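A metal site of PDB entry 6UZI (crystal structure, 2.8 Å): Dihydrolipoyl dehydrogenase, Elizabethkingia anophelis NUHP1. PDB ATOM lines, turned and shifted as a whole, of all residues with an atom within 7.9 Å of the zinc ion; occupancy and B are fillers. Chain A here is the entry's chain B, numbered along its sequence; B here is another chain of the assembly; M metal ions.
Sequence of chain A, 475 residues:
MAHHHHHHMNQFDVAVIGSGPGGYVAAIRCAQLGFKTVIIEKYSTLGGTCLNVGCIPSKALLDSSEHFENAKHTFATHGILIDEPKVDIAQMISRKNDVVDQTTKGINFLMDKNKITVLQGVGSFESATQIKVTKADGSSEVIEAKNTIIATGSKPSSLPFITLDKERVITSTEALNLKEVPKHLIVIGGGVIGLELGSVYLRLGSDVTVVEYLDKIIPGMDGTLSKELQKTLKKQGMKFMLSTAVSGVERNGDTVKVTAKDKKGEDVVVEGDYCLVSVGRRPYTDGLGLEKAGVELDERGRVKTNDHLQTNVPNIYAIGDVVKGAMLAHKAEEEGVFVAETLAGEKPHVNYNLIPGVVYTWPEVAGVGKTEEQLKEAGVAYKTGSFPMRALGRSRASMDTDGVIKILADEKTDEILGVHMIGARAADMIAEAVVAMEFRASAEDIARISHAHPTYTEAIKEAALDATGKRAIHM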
ATOM      1  N   LEU A 392     -16.574   1.984  35.951  1.00  0.00           N
ATOM      2  CA  LEU A 392     -16.654   1.205  34.716  1.00  0.00           C
ATOM      3  C   LEU A 392     -16.320  -0.249  34.991  1.00  0.00           C
ATOM      4  O   LEU A 392     -15.377  -0.555  35.715  1.00  0.00           O
ATOM      5  CB  LEU A 392     -15.693   1.739  33.667  1.00  0.00           C
ATOM      6  CG  LEU A 392     -15.952   3.136  33.094  1.00  0.00           C
ATOM      7  CD1 LEU A 392     -14.877   3.458  32.096  1.00  0.00           C
ATOM      8  CD2 LEU A 392     -17.314   3.213  32.452  1.00  0.00           C
ATOM      9  N   GLY A 393     -17.117  -1.148  34.401  1.00  0.00           N
ATOM     10  CA  GLY A 393     -16.799  -2.568  34.493  1.00  0.00           C
ATOM     11  C   GLY A 393     -15.463  -2.906  33.862  1.00  0.00           C
ATOM     12  O   GLY A 393     -14.710  -3.736  34.387  1.00  0.00           O
ATOM     13  N   HIS A 451     -21.838   3.481  22.432  1.00  0.00           N
ATOM     14  CA  HIS A 451     -20.479   3.238  22.908  1.00  0.00           C
ATOM     15  C   HIS A 451     -20.332   1.756  23.254  1.00  0.00           C
ATOM     16  O   HIS A 451     -21.111   1.214  24.039  1.00  0.00           O
ATOM     17  CB  HIS A 451     -20.151   4.140  24.099  1.00  0.00           C
ATOM     18  CG  HIS A 451     -19.981   5.580  23.732  1.00  0.00           C
ATOM     19  ND1 HIS A 451     -20.984   6.330  23.166  1.00  0.00           N
ATOM     20  CD2 HIS A 451     -18.924   6.414  23.874  1.00  0.00           C
ATOM     21  CE1 HIS A 451     -20.555   7.558  22.957  1.00  0.00           C
ATOM     22  NE2 HIS A 451     -19.306   7.638  23.382  1.00  0.00           N
ATOM     23  N   ALA A 452     -19.313   1.118  22.675  1.00  0.00           N
ATOM     24  CA  ALA A 452     -19.100  -0.305  22.875  1.00  0.00           C
ATOM     25  C   ALA A 452     -19.016  -0.637  24.361  1.00  0.00           C
ATOM     26  O   ALA A 452     -18.455   0.116  25.149  1.00  0.00           O
ATOM     27  CB  ALA A 452     -17.822  -0.766  22.166  1.00  0.00           C
ATOM     28  N   HIS A 453     -19.623  -1.765  24.734  1.00  0.00           N
ATOM     29  CA  HIS A 453     -19.613  -2.261  26.100  1.00  0.00           C
ATOM     30  C   HIS A 453     -18.932  -3.618  26.165  1.00  0.00           C
ATOM     31  O   HIS A 453     -19.251  -4.510  25.366  1.00  0.00           O
ATOM     32  CB  HIS A 453     -21.043  -2.361  26.647  1.00  0.00           C
ATOM     33  CG  HIS A 453     -21.106  -2.875  28.045  1.00  0.00           C
ATOM     34  ND1 HIS A 453     -21.261  -2.043  29.138  1.00  0.00           N
ATOM     35  CD2 HIS A 453     -21.073  -4.130  28.540  1.00  0.00           C
ATOM     36  CE1 HIS A 453     -21.292  -2.767  30.243  1.00  0.00           C
ATOM     37  NE2 HIS A 453     -21.182  -4.034  29.910  1.00  0.00           N
ATOM     38  N   PRO A 454     -17.977  -3.818  27.082  1.00  0.00           N
ATOM     39  CA  PRO A 454     -17.433  -2.819  28.005  1.00  0.00           C
ATOM     40  C   PRO A 454     -16.168  -2.122  27.490  1.00  0.00           C
ATOM     41  O   PRO A 454     -15.220  -2.792  27.129  1.00  0.00           O
ATOM     42  CB  PRO A 454     -17.095  -3.655  29.245  1.00  0.00           C
ATOM     43  CG  PRO A 454     -16.699  -4.981  28.682  1.00  0.00           C
ATOM     44  CD  PRO A 454     -17.525  -5.183  27.425  1.00  0.00           C
ATOM     45  N   THR A 455     -16.153  -0.784  27.461  1.00  0.00           N
ATOM     46  CA  THR A 455     -14.965  -0.036  27.081  1.00  0.00           C
ATOM     47  C   THR A 455     -14.801   1.160  27.993  1.00  0.00           C
ATOM     48  O   THR A 455     -15.712   1.563  28.717  1.00  0.00           O
ATOM     49  CB  THR A 455     -15.010   0.439  25.612  1.00  0.00           C
ATOM     50  OG1 THR A 455     -16.174   1.265  25.407  1.00  0.00           O
ATOM     51  CG2 THR A 455     -14.998  -0.740  24.645  1.00  0.00           C
ATOM     52  N   GLU A 458     -17.085   4.334  27.516  1.00  0.00           N
ATOM     53  CA  GLU A 458     -18.412   4.462  28.121  1.00  0.00           C
ATOM     54  C   GLU A 458     -18.432   5.558  29.175  1.00  0.00           C
ATOM     55  O   GLU A 458     -19.504   6.119  29.461  1.00  0.00           O
ATOM     56  CB  GLU A 458     -18.842   3.123  28.729  1.00  0.00           C
ATOM     57  CG  GLU A 458     -18.932   1.976  27.727  1.00  0.00           C
ATOM     58  CD  GLU A 458     -19.718   0.798  28.263  1.00  0.00           C
ATOM     59  OE1 GLU A 458     -20.956   0.773  28.088  1.00  0.00           O
ATOM     60  OE2 GLU A 458     -19.090  -0.106  28.864  1.00  0.00           O
ATOM     61  N   LYS A 461     -19.554   8.648  27.367  1.00  0.00           N
ATOM     62  CA  LYS A 461     -21.005   8.675  27.189  1.00  0.00           C
ATOM     63  C   LYS A 461     -21.700   9.031  28.502  1.00  0.00           C
ATOM     64  O   LYS A 461     -22.640   9.821  28.520  1.00  0.00           O
ATOM     65  CB  LYS A 461     -21.486   7.320  26.653  1.00  0.00           C
ATOM     66  CG  LYS A 461     -22.991   7.190  26.546  1.00  0.00           C
ATOM     67  CD  LYS A 461     -23.393   5.740  26.468  1.00  0.00           C
ATOM     68  CE  LYS A 461     -24.880   5.564  26.222  1.00  0.00           C
ATOM     69  NZ  LYS A 461     -25.263   5.997  24.862  1.00  0.00           N
ATOM     70  N   GLU A 462     -21.227   8.462  29.617  1.00  0.00           N
ATOM     71  CA  GLU A 462     -21.845   8.726  30.903  1.00  0.00           C
ATOM     72  C   GLU A 462     -21.611  10.172  31.342  1.00  0.00           C
ATOM     73  O   GLU A 462     -22.529  10.821  31.834  1.00  0.00           O
ATOM     74  CB  GLU A 462     -21.309   7.762  31.954  1.00  0.00           C
ATOM     75  CG  GLU A 462     -21.719   6.305  31.770  1.00  0.00           C
ATOM     76  CD  GLU A 462     -23.204   6.066  32.016  1.00  0.00           C
ATOM     77  OE1 GLU A 462     -23.745   6.688  32.944  1.00  0.00           O
ATOM     78  OE2 GLU A 462     -23.804   5.248  31.304  1.00  0.00           O
ATOM     79  N   ILE A 473     -26.468   7.088  33.745  1.00  0.00           N
ATOM     80  CA  ILE A 473     -27.134   5.817  34.025  1.00  0.00           C
ATOM     81  C   ILE A 473     -26.413   5.020  35.114  1.00  0.00           C
ATOM     82  O   ILE A 473     -27.051   4.448  35.999  1.00  0.00           O
ATOM     83  CB  ILE A 473     -27.263   4.996  32.726  1.00  0.00           C
ATOM     84  CG1 ILE A 473     -28.183   5.722  31.746  1.00  0.00           C
ATOM     85  CG2 ILE A 473     -27.741   3.580  33.018  1.00  0.00           C
ATOM     86  CD1 ILE A 473     -29.648   5.683  32.149  1.00  0.00           C
ATOM     87  N   HIS A 474     -25.078   4.948  35.066  1.00  0.00           N
ATOM     88  CA  HIS A 474     -24.312   4.070  35.932  1.00  0.00           C
ATOM     89  C   HIS A 474     -23.670   4.800  37.102  1.00  0.00           C
ATOM     90  O   HIS A 474     -22.685   4.320  37.668  1.00  0.00           O
ATOM     91  CB  HIS A 474     -23.260   3.321  35.118  1.00  0.00           C
ATOM     92  CG  HIS A 474     -23.849   2.370  34.117  1.00  0.00           C
ATOM     93  ND1 HIS A 474     -24.272   2.787  32.863  1.00  0.00           N
ATOM     94  CD2 HIS A 474     -24.125   1.048  34.193  1.00  0.00           C
ATOM     95  CE1 HIS A 474     -24.764   1.745  32.211  1.00  0.00           C
ATOM     96  NE2 HIS A 474     -24.682   0.678  32.994  1.00  0.00           N
ATOM     97  N   PRO B  21     -27.734  -6.066  30.883  1.00  0.00           N
ATOM     98  CA  PRO B  21     -27.454  -4.657  30.557  1.00  0.00           C
ATOM     99  C   PRO B  21     -28.630  -3.931  29.923  1.00  0.00           C
ATOM    100  O   PRO B  21     -28.892  -2.778  30.271  1.00  0.00           O
ATOM    101  CB  PRO B  21     -26.255  -4.757  29.599  1.00  0.00           C
ATOM    102  CG  PRO B  21     -25.615  -6.045  29.951  1.00  0.00           C
ATOM    103  CD  PRO B  21     -26.740  -6.977  30.298  1.00  0.00           C
ATOM    104  N   TYR B  24     -31.546  -3.619  33.136  1.00  0.00           N
ATOM    105  CA  TYR B  24     -31.398  -2.691  34.248  1.00  0.00           C
ATOM    106  C   TYR B  24     -31.130  -1.259  33.766  1.00  0.00           C
ATOM    107  O   TYR B  24     -31.478  -0.303  34.467  1.00  0.00           O
ATOM    108  CB  TYR B  24     -30.321  -3.193  35.214  1.00  0.00           C
ATOM    109  CG  TYR B  24     -28.880  -2.905  34.853  1.00  0.00           C
ATOM    110  CD1 TYR B  24     -28.284  -1.695  35.163  1.00  0.00           C
ATOM    111  CD2 TYR B  24     -28.097  -3.885  34.256  1.00  0.00           C
ATOM    112  CE1 TYR B  24     -26.962  -1.439  34.849  1.00  0.00           C
ATOM    113  CE2 TYR B  24     -26.774  -3.639  33.942  1.00  0.00           C
ATOM    114  CZ  TYR B  24     -26.209  -2.422  34.242  1.00  0.00           C
ATOM    115  OH  TYR B  24     -24.886  -2.176  33.928  1.00  0.00           O
ATOM    116  N   VAL B  25     -30.535  -1.086  32.589  1.00  0.00           N
ATOM    117  CA  VAL B  25     -30.440   0.262  32.047  1.00  0.00           C
ATOM    118  C   VAL B  25     -31.823   0.782  31.679  1.00  0.00           C
ATOM    119  O   VAL B  25     -32.169   1.928  31.989  1.00  0.00           O
ATOM    120  CB  VAL B  25     -29.469   0.309  30.862  1.00  0.00           C
ATOM    121  CG1 VAL B  25     -29.622   1.591  30.071  1.00  0.00           C
ATOM    122  CG2 VAL B  25     -28.036   0.162  31.363  1.00  0.00           C
ATOM    123  N   CYS B  50     -23.919 -10.635  30.751  1.00  0.00           N
ATOM    124  CA  CYS B  50     -22.702  -9.849  30.545  1.00  0.00           C
ATOM    125  C   CYS B  50     -21.864  -9.757  31.813  1.00  0.00           C
ATOM    126  O   CYS B  50     -20.626  -9.797  31.759  1.00  0.00           O
ATOM    127  CB  CYS B  50     -23.078  -8.464  30.047  1.00  0.00           C
ATOM    128  SG  CYS B  50     -21.696  -7.357  29.656  1.00  0.00           S
ATOM    129  N   ALA B 329     -24.012  -6.084  24.088  1.00  0.00           N
ATOM    130  CA  ALA B 329     -24.465  -5.534  25.359  1.00  0.00           C
ATOM    131  C   ALA B 329     -24.882  -4.071  25.212  1.00  0.00           C
ATOM    132  O   ALA B 329     -25.908  -3.653  25.753  1.00  0.00           O
ATOM    133  CB  ALA B 329     -23.375  -5.696  26.428  1.00  0.00           C
ATOM    134  N   HIS B 330     -24.069  -3.268  24.524  1.00  0.00           N
ATOM    135  CA  HIS B 330     -24.456  -1.872  24.343  1.00  0.00           C
ATOM    136  C   HIS B 330     -25.642  -1.721  23.389  1.00  0.00           C
ATOM    137  O   HIS B 330     -26.342  -0.711  23.466  1.00  0.00           O
ATOM    138  CB  HIS B 330     -23.272  -1.031  23.857  1.00  0.00           C
ATOM    139  CG  HIS B 330     -22.558  -1.610  22.674  1.00  0.00           C
ATOM    140  ND1 HIS B 330     -21.816  -2.771  22.740  1.00  0.00           N
ATOM    141  CD2 HIS B 330     -22.448  -1.166  21.404  1.00  0.00           C
ATOM    142  CE1 HIS B 330     -21.289  -3.026  21.561  1.00  0.00           C
ATOM    143  NE2 HIS B 330     -21.662  -2.074  20.729  1.00  0.00           N
ATOM    144  N   GLU B 333     -28.444  -2.042  25.833  1.00  0.00           N
ATOM    145  CA  GLU B 333     -28.526  -0.814  26.604  1.00  0.00           C
ATOM    146  C   GLU B 333     -29.256   0.276  25.821  1.00  0.00           C
ATOM    147  O   GLU B 333     -30.136   0.958  26.357  1.00  0.00           O
ATOM    148  CB  GLU B 333     -27.123  -0.368  26.988  1.00  0.00           C
ATOM    149  CG  GLU B 333     -26.552  -1.071  28.187  1.00  0.00           C
ATOM    150  CD  GLU B 333     -25.087  -0.747  28.431  1.00  0.00           C
ATOM    151  OE1 GLU B 333     -24.419  -0.262  27.498  1.00  0.00           O
ATOM    152  OE2 GLU B 333     -24.615  -0.955  29.565  1.00  0.00           O
HETATM  153 ZN    ZN M   1     -22.518  -0.261  29.324  1.00  0.00          ZN
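The backbone NH of His 453 is in hydrogen-bond range of a ring nitrogen (ND1) of His 330 of chain B (3.1 Å).
The side-chain sulfur of Cys 50 of chain B is in hydrogen-bond range of a ring nitrogen (NE2) of His 453, 3.4 Å away.
The backbone NH of Thr 455 is in hydrogen-bond range of the side-chain carboxylate of Glu 458, 3.3 Å away.
ND1 of His 453 binds the zinc ion (2.2 Å).
The zinc ion is bound by the side-chain carboxylate (OE2) of Glu 333 of chain B, 2.2 Å away.
OE1 of Glu 458 is bound to the zinc ion (2.2 Å).
Slightly farther from the zinc ion lies the side-chain carboxylate (OE1) of Glu 333 of chain B (2.6 Å).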
